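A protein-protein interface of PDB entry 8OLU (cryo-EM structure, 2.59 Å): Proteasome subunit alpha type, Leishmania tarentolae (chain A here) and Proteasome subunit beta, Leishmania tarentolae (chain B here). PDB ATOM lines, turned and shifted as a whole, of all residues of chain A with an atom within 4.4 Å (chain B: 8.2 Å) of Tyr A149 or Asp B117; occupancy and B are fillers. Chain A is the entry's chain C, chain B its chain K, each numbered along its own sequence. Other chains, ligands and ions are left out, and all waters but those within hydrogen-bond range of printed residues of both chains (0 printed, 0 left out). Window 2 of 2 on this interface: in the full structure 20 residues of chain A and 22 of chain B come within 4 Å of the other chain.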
ATOM      1  N   TRP A 145     -28.562   6.586 -26.728  1.00  0.00           N
ATOM      2  CA  TRP A 145     -28.559   5.631 -27.785  1.00  0.00           C
ATOM      3  C   TRP A 145     -27.142   5.485 -28.262  1.00  0.00           C
ATOM      4  O   TRP A 145     -26.421   6.456 -28.366  1.00  0.00           O
ATOM      5  CB  TRP A 145     -29.504   6.102 -28.853  1.00  0.00           C
ATOM      6  CG  TRP A 145     -29.487   5.119 -29.968  1.00  0.00           C
ATOM      7  CD1 TRP A 145     -30.360   4.090 -30.168  1.00  0.00           C
ATOM      8  CD2 TRP A 145     -28.484   5.029 -30.984  1.00  0.00           C
ATOM      9  NE1 TRP A 145     -29.962   3.364 -31.246  1.00  0.00           N
ATOM     10  CE2 TRP A 145     -28.831   3.926 -31.784  1.00  0.00           C
ATOM     11  CE3 TRP A 145     -27.346   5.772 -31.301  1.00  0.00           C
ATOM     12  CZ2 TRP A 145     -28.066   3.543 -32.888  1.00  0.00           C
ATOM     13  CZ3 TRP A 145     -26.605   5.416 -32.407  1.00  0.00           C
ATOM     14  CH2 TRP A 145     -26.950   4.299 -33.168  1.00  0.00           C
ATOM     15  N   ASP A 146     -26.698   4.266 -28.425  1.00  0.00           N
ATOM     16  CA  ASP A 146     -25.377   4.061 -28.979  1.00  0.00           C
ATOM     17  C   ASP A 146     -25.498   2.877 -29.887  1.00  0.00           C
ATOM     18  O   ASP A 146     -26.475   2.154 -29.849  1.00  0.00           O
ATOM     19  CB  ASP A 146     -24.321   3.884 -27.881  1.00  0.00           C
ATOM     20  CG  ASP A 146     -24.529   2.722 -26.911  1.00  0.00           C
ATOM     21  OD1 ASP A 146     -25.026   1.698 -27.372  1.00  0.00           O
ATOM     22  OD2 ASP A 146     -24.181   2.842 -25.678  1.00  0.00           O
ATOM     23  N   ARG A 147     -24.502   2.656 -30.699  1.00  0.00           N
ATOM     24  CA  ARG A 147     -24.634   1.602 -31.701  1.00  0.00           C
ATOM     25  C   ARG A 147     -24.468   0.212 -31.063  1.00  0.00           C
ATOM     26  O   ARG A 147     -24.803  -0.778 -31.677  1.00  0.00           O
ATOM     27  CB  ARG A 147     -23.623   1.906 -32.799  1.00  0.00           C
ATOM     28  CG  ARG A 147     -22.196   1.655 -32.329  1.00  0.00           C
ATOM     29  CD  ARG A 147     -21.282   2.703 -32.960  1.00  0.00           C
ATOM     30  NE  ARG A 147     -19.962   2.139 -33.177  1.00  0.00           N
ATOM     31  CZ  ARG A 147     -19.695   1.347 -34.200  1.00  0.00           C
ATOM     32  NH1 ARG A 147     -20.310   1.581 -35.360  1.00  0.00           N
ATOM     33  NH2 ARG A 147     -18.858   0.329 -34.022  1.00  0.00           N
ATOM     34  N   TYR A 148     -24.015   0.137 -29.823  1.00  0.00           N
ATOM     35  CA  TYR A 148     -23.699  -1.125 -29.194  1.00  0.00           C
ATOM     36  C   TYR A 148     -24.959  -1.778 -28.649  1.00  0.00           C
ATOM     37  O   TYR A 148     -25.133  -2.988 -28.745  1.00  0.00           O
ATOM     38  CB  TYR A 148     -22.689  -0.952 -28.059  1.00  0.00           C
ATOM     39  CG  TYR A 148     -21.374  -0.355 -28.488  1.00  0.00           C
ATOM     40  CD1 TYR A 148     -20.448  -1.103 -29.211  1.00  0.00           C
ATOM     41  CD2 TYR A 148     -21.048   0.971 -28.201  1.00  0.00           C
ATOM     42  CE1 TYR A 148     -19.228  -0.563 -29.602  1.00  0.00           C
ATOM     43  CE2 TYR A 148     -19.832   1.519 -28.583  1.00  0.00           C
ATOM     44  CZ  TYR A 148     -18.920   0.751 -29.288  1.00  0.00           C
ATOM     45  OH  TYR A 148     -17.716   1.281 -29.686  1.00  0.00           O
ATOM     46  N   TYR A 149     -25.835  -0.987 -28.079  1.00  0.00           N
ATOM     47  CA  TYR A 149     -26.914  -1.533 -27.281  1.00  0.00           C
ATOM     48  C   TYR A 149     -28.227  -0.874 -27.626  1.00  0.00           C
ATOM     49  O   TYR A 149     -29.228  -1.313 -27.121  1.00  0.00           O
ATOM     50  CB  TYR A 149     -26.553  -1.400 -25.815  1.00  0.00           C
ATOM     51  CG  TYR A 149     -25.527  -2.433 -25.408  1.00  0.00           C
ATOM     52  CD1 TYR A 149     -25.796  -3.798 -25.502  1.00  0.00           C
ATOM     53  CD2 TYR A 149     -24.277  -2.066 -24.926  1.00  0.00           C
ATOM     54  CE1 TYR A 149     -24.852  -4.756 -25.149  1.00  0.00           C
ATOM     55  CE2 TYR A 149     -23.321  -3.008 -24.566  1.00  0.00           C
ATOM     56  CZ  TYR A 149     -23.601  -4.358 -24.692  1.00  0.00           C
ATOM     57  OH  TYR A 149     -22.633  -5.276 -24.322  1.00  0.00           O
ATOM     58  N   GLY A 150     -28.227   0.132 -28.491  1.00  0.00           N
ATOM     59  CA  GLY A 150     -29.445   0.844 -28.800  1.00  0.00           C
ATOM     60  C   GLY A 150     -29.901   1.771 -27.686  1.00  0.00           C
ATOM     61  O   GLY A 150     -29.108   2.259 -26.896  1.00  0.00           O
ATOM     62  N   TYR A 151     -31.194   2.028 -27.629  1.00  0.00           N
ATOM     63  CA  TYR A 151     -31.746   2.794 -26.544  1.00  0.00           C
ATOM     64  C   TYR A 151     -31.433   2.086 -25.244  1.00  0.00           C
ATOM     65  O   TYR A 151     -31.623   0.884 -25.120  1.00  0.00           O
ATOM     66  CB  TYR A 151     -33.231   2.965 -26.763  1.00  0.00           C
ATOM     67  CG  TYR A 151     -33.500   3.717 -28.033  1.00  0.00           C
ATOM     68  CD1 TYR A 151     -33.227   5.067 -28.166  1.00  0.00           C
ATOM     69  CD2 TYR A 151     -33.895   3.054 -29.171  1.00  0.00           C
ATOM     70  CE1 TYR A 151     -33.474   5.749 -29.351  1.00  0.00           C
ATOM     71  CE2 TYR A 151     -34.132   3.713 -30.369  1.00  0.00           C
ATOM     72  CZ  TYR A 151     -33.949   5.074 -30.458  1.00  0.00           C
ATOM     73  OH  TYR A 151     -34.196   5.651 -31.694  1.00  0.00           O
ATOM     74  N   GLN A 152     -30.925   2.868 -24.309  1.00  0.00           N
ATOM     75  CA  GLN A 152     -30.588   2.432 -22.985  1.00  0.00           C
ATOM     76  C   GLN A 152     -31.152   3.411 -21.983  1.00  0.00           C
ATOM     77  O   GLN A 152     -31.543   4.512 -22.322  1.00  0.00           O
ATOM     78  CB  GLN A 152     -29.088   2.435 -22.887  1.00  0.00           C
ATOM     79  CG  GLN A 152     -28.430   1.247 -23.589  1.00  0.00           C
ATOM     80  CD  GLN A 152     -27.035   1.572 -24.089  1.00  0.00           C
ATOM     81  OE1 GLN A 152     -26.036   1.348 -23.382  1.00  0.00           O
ATOM     82  NE2 GLN A 152     -26.961   2.176 -25.280  1.00  0.00           N
ATOM     83  N   LYS A 223     -34.201   8.555 -32.376  1.00  0.00           N
ATOM     84  CA  LYS A 223     -33.425   8.820 -33.576  1.00  0.00           C
ATOM     85  C   LYS A 223     -34.314   9.504 -34.592  1.00  0.00           C
ATOM     86  O   LYS A 223     -35.489   9.213 -34.677  1.00  0.00           O
ATOM     87  CB  LYS A 223     -32.757   7.537 -34.064  1.00  0.00           C
ATOM     88  CG  LYS A 223     -31.627   7.078 -33.146  1.00  0.00           C
ATOM     89  CD  LYS A 223     -30.568   6.296 -33.876  1.00  0.00           C
ATOM     90  CE  LYS A 223     -31.087   4.935 -34.286  1.00  0.00           C
ATOM     91  NZ  LYS A 223     -30.218   4.327 -35.320  1.00  0.00           N
ATOM     92  N   ARG B  69     -12.021  -2.888 -24.645  1.00  0.00           N
ATOM     93  CA  ARG B  69     -12.961  -3.910 -25.049  1.00  0.00           C
ATOM     94  C   ARG B  69     -13.405  -4.710 -23.810  1.00  0.00           C
ATOM     95  O   ARG B  69     -14.490  -5.300 -23.829  1.00  0.00           O
ATOM     96  CB  ARG B  69     -12.237  -4.707 -26.139  1.00  0.00           C
ATOM     97  CG  ARG B  69     -13.041  -5.765 -26.866  1.00  0.00           C
ATOM     98  CD  ARG B  69     -12.261  -6.588 -27.880  1.00  0.00           C
ATOM     99  NE  ARG B  69     -11.039  -7.162 -27.294  1.00  0.00           N
ATOM    100  CZ  ARG B  69      -9.780  -6.815 -27.600  1.00  0.00           C
ATOM    101  NH1 ARG B  69      -8.779  -7.550 -27.142  1.00  0.00           N
ATOM    102  NH2 ARG B  69      -9.526  -5.751 -28.356  1.00  0.00           N
ATOM    103  N   GLN B  72     -15.968  -2.749 -21.729  1.00  0.00           N
ATOM    104  CA  GLN B  72     -17.033  -2.503 -22.661  1.00  0.00           C
ATOM    105  C   GLN B  72     -17.545  -3.856 -23.156  1.00  0.00           C
ATOM    106  O   GLN B  72     -17.975  -3.994 -24.300  1.00  0.00           O
ATOM    107  CB  GLN B  72     -16.552  -1.641 -23.850  1.00  0.00           C
ATOM    108  CG  GLN B  72     -16.034  -0.211 -23.508  1.00  0.00           C
ATOM    109  CD  GLN B  72     -15.513   0.670 -24.644  1.00  0.00           C
ATOM    110  OE1 GLN B  72     -15.818   0.456 -25.821  1.00  0.00           O
ATOM    111  NE2 GLN B  72     -14.729   1.691 -24.294  1.00  0.00           N
ATOM    112  N   HIS B  73     -17.437  -4.872 -22.285  1.00  0.00           N
ATOM    113  CA  HIS B  73     -18.181  -6.121 -22.385  1.00  0.00           C
ATOM    114  C   HIS B  73     -18.099  -6.690 -23.789  1.00  0.00           C
ATOM    115  O   HIS B  73     -19.097  -7.153 -24.317  1.00  0.00           O
ATOM    116  CB  HIS B  73     -19.618  -5.922 -21.847  1.00  0.00           C
ATOM    117  CG  HIS B  73     -19.584  -5.283 -20.485  1.00  0.00           C
ATOM    118  ND1 HIS B  73     -18.698  -5.661 -19.495  1.00  0.00           N
ATOM    119  CD2 HIS B  73     -20.212  -4.165 -20.019  1.00  0.00           C
ATOM    120  CE1 HIS B  73     -18.829  -4.861 -18.436  1.00  0.00           C
ATOM    121  NE2 HIS B  73     -19.760  -3.919 -18.744  1.00  0.00           N
ATOM    122  N   GLY B  74     -16.880  -6.686 -24.355  1.00  0.00           N
ATOM    123  CA  GLY B  74     -16.529  -7.560 -25.474  1.00  0.00           C
ATOM    124  C   GLY B  74     -16.765  -6.945 -26.850  1.00  0.00           C
ATOM    125  O   GLY B  74     -16.597  -7.606 -27.868  1.00  0.00           O
ATOM    126  N   ARG B  75     -17.118  -5.662 -26.863  1.00  0.00           N
ATOM    127  CA  ARG B  75     -17.551  -4.951 -28.048  1.00  0.00           C
ATOM    128  C   ARG B  75     -16.337  -4.387 -28.762  1.00  0.00           C
ATOM    129  O   ARG B  75     -15.509  -3.713 -28.145  1.00  0.00           O
ATOM    130  CB  ARG B  75     -18.312  -3.683 -27.648  1.00  0.00           C
ATOM    131  CG  ARG B  75     -19.654  -3.889 -26.962  1.00  0.00           C
ATOM    132  CD  ARG B  75     -19.999  -2.809 -25.922  1.00  0.00           C
ATOM    133  NE  ARG B  75     -19.300  -1.519 -25.951  1.00  0.00           N
ATOM    134  CZ  ARG B  75     -19.421  -0.581 -25.008  1.00  0.00           C
ATOM    135  NH1 ARG B  75     -20.339  -0.693 -24.063  1.00  0.00           N
ATOM    136  NH2 ARG B  75     -18.611   0.466 -25.006  1.00  0.00           N
ATOM    137  N   PRO B 113     -21.107  -4.697 -38.562  1.00  0.00           N
ATOM    138  CA  PRO B 113     -22.140  -4.348 -37.576  1.00  0.00           C
ATOM    139  C   PRO B 113     -21.776  -4.907 -36.206  1.00  0.00           C
ATOM    140  O   PRO B 113     -21.490  -6.093 -36.058  1.00  0.00           O
ATOM    141  CB  PRO B 113     -23.377  -5.021 -38.140  1.00  0.00           C
ATOM    142  CG  PRO B 113     -23.112  -5.041 -39.631  1.00  0.00           C
ATOM    143  CD  PRO B 113     -21.646  -5.381 -39.744  1.00  0.00           C
ATOM    144  N   VAL B 114     -21.727  -4.037 -35.205  1.00  0.00           N
ATOM    145  CA  VAL B 114     -21.292  -4.462 -33.882  1.00  0.00           C
ATOM    146  C   VAL B 114     -22.479  -5.046 -33.114  1.00  0.00           C
ATOM    147  O   VAL B 114     -22.283  -5.889 -32.239  1.00  0.00           O
ATOM    148  CB  VAL B 114     -20.594  -3.317 -33.133  1.00  0.00           C
ATOM    149  CG1 VAL B 114     -21.589  -2.279 -32.658  1.00  0.00           C
ATOM    150  CG2 VAL B 114     -19.783  -3.855 -31.976  1.00  0.00           C
ATOM    151  N   SER B 115     -23.690  -4.661 -33.550  1.00  0.00           N
ATOM    152  CA  SER B 115     -24.935  -5.166 -33.013  1.00  0.00           C
ATOM    153  C   SER B 115     -26.046  -5.031 -34.057  1.00  0.00           C
ATOM    154  O   SER B 115     -25.772  -4.645 -35.182  1.00  0.00           O
ATOM    155  CB  SER B 115     -25.253  -4.412 -31.729  1.00  0.00           C
ATOM    156  OG  SER B 115     -25.907  -3.154 -31.962  1.00  0.00           O
ATOM    157  N   GLU B 116     -27.303  -5.310 -33.661  1.00  0.00           N
ATOM    158  CA  GLU B 116     -28.476  -5.134 -34.514  1.00  0.00           C
ATOM    159  C   GLU B 116     -28.769  -3.652 -34.768  1.00  0.00           C
ATOM    160  O   GLU B 116     -29.393  -3.297 -35.771  1.00  0.00           O
ATOM    161  CB  GLU B 116     -29.707  -5.763 -33.863  1.00  0.00           C
ATOM    162  CG  GLU B 116     -29.587  -7.269 -33.630  1.00  0.00           C
ATOM    163  CD  GLU B 116     -30.836  -7.954 -33.078  1.00  0.00           C
ATOM    164  OE1 GLU B 116     -31.896  -7.883 -33.743  1.00  0.00           O
ATOM    165  OE2 GLU B 116     -30.754  -8.571 -31.984  1.00  0.00           O
ATOM    166  N   ASP B 117     -28.304  -2.789 -33.854  1.00  0.00           N
ATOM    167  CA  ASP B 117     -28.653  -1.373 -33.829  1.00  0.00           C
ATOM    168  C   ASP B 117     -27.661  -0.547 -34.653  1.00  0.00           C
ATOM    169  O   ASP B 117     -28.015   0.551 -35.086  1.00  0.00           O
ATOM    170  CB  ASP B 117     -28.791  -0.886 -32.378  1.00  0.00           C
ATOM    171  CG  ASP B 117     -29.903  -1.592 -31.599  1.00  0.00           C
ATOM    172  OD1 ASP B 117     -31.047  -1.580 -32.097  1.00  0.00           O
ATOM    173  OD2 ASP B 117     -29.622  -2.168 -30.500  1.00  0.00           O
ATOM    174  N   ASP B 118     -26.474  -1.114 -34.934  1.00  0.00           N
ATOM    175  CA  ASP B 118     -25.380  -0.404 -35.587  1.00  0.00           C
ATOM    176  C   ASP B 118     -25.790  -0.019 -37.016  1.00  0.00           C
ATOM    177  O   ASP B 118     -25.946  -0.851 -37.903  1.00  0.00           O
ATOM    178  CB  ASP B 118     -24.048  -1.182 -35.478  1.00  0.00           C
ATOM    179  CG  ASP B 118     -22.757  -0.375 -35.716  1.00  0.00           C
ATOM    180  OD1 ASP B 118     -22.835   0.824 -36.155  1.00  0.00           O
ATOM    181  OD2 ASP B 118     -21.651  -0.926 -35.460  1.00  0.00           O
ATOM    182  N   ASP B 119     -25.972   1.292 -37.199  1.00  0.00           N
ATOM    183  CA  ASP B 119     -26.301   1.890 -38.484  1.00  0.00           C
ATOM    184  C   ASP B 119     -25.007   2.359 -39.156  1.00  0.00           C
ATOM    185  O   ASP B 119     -25.054   3.050 -40.171  1.00  0.00           O
ATOM    186  CB  ASP B 119     -27.281   3.063 -38.292  1.00  0.00           C
ATOM    187  CG  ASP B 119     -26.856   4.102 -37.243  1.00  0.00           C
ATOM    188  OD1 ASP B 119     -25.784   3.893 -36.581  1.00  0.00           O
ATOM    189  OD2 ASP B 119     -27.603   5.129 -37.086  1.00  0.00           O
ATOM    190  N   GLY B 120     -23.867   1.985 -38.554  1.00  0.00           N
ATOM    191  CA  GLY B 120     -22.574   2.572 -38.873  1.00  0.00           C
ATOM    192  C   GLY B 120     -22.046   2.098 -40.220  1.00  0.00           C
ATOM    193  O   GLY B 120     -22.748   1.460 -41.008  1.00  0.00           O
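O of Arg A147 lies within hydrogen-bond range of OG of Ser B115 (2.6 Å). The backbone carbonyl oxygen (O) of Tyr A148 lies close to the side-chain hydroxyl (OG) of Ser B115, 3.3 Å away. OD2 of Asp B117 sits at hydrogen-bond distance from N of Gly A150, 3.4 Å away. The side-chain carboxylate of Asp B118 is in salt-bridge range of the guanidinium group of Arg A147 (2.8 Å). OD2 of Asp B119 is in salt-bridge range of NZ of Lys A223 (3.3 Å).
Of the 13 printed residues of chain B, 7 touch a printed residue of chain A. Printed residues of chain B that touch a printed residue of chain A: His B73, Arg B75, Val B114, Ser B115, Asp B117, Asp B118 and Asp B119. Along chain B the printed residues that touch a printed residue of chain A span positions 73 to 119. Hydrophobic or aromatic side chains of chain A within 4 Å of the printed part of chain B: Trp A145, Tyr A148 and Tyr A149. Along chain A the printed residues that touch a printed residue of chain B span positions 145 to 223. Among the printed residues, 13 pairs touch across the chains. Among the printed residues, Asp or Glu carboxylates within 4 Å of a Lys or Arg side-chain nitrogen of the other chain: Arg A147 with Asp B118 and Lys A223 with Asp B119.
Among the printed residues, merely in contact across the chains: Tyr A149 with Asp B117 (3.4 Å), Tyr A148 with Arg B75 (3.5 Å), Tyr A149 with Arg B75 (3.6 Å), Trp A145 with Asp B119 (3.6 Å), Arg A147 with Val B114 (3.7 Å), Trp A145 with Asp B117 (3.7 Å), Tyr A148 with Val B114 (3.8 Å) and Tyr A149 with His B73 (3.95 Å).
Tyr A149 touches just these residues of chain B: His B73, Arg B75 and Asp B117. Printed residues of chain A within 4 Å of Val B114: Arg A147 and Tyr A148. Of the printed residues of chain A, His B73 touches Tyr A149 (3.95 Å). The nearest residue of chain B that does not touch Tyr A149 is Ser B115 (4.4 Å). The nearest printed residue of chain A that does not touch Arg B75 is Asp A146 (5.5 Å).
OE1 of Gln B72 sits at hydrogen-bond distance from NH2 of Arg B75 (2.9 Å). The side-chain hydroxyl (OG) of Ser B115 lies within hydrogen-bond range of the backbone NH (N) of Asp B117 (3.1 Å). OD1 of Asp B118 lies within hydrogen-bond range of N of Gly B120, 2.9 Å away. The side-chain carboxylate (OD1) of Asp A146 is in hydrogen-bond range of the backbone NH (N) of Tyr A148 (3.1 Å). NE2 of Gln A152 is in hydrogen-bond range of O of Gly A150 (2.7 Å). The backbone NH of Lys A223 lies within hydrogen-bond range of the side-chain hydroxyl of Tyr A151 (3.0 Å).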
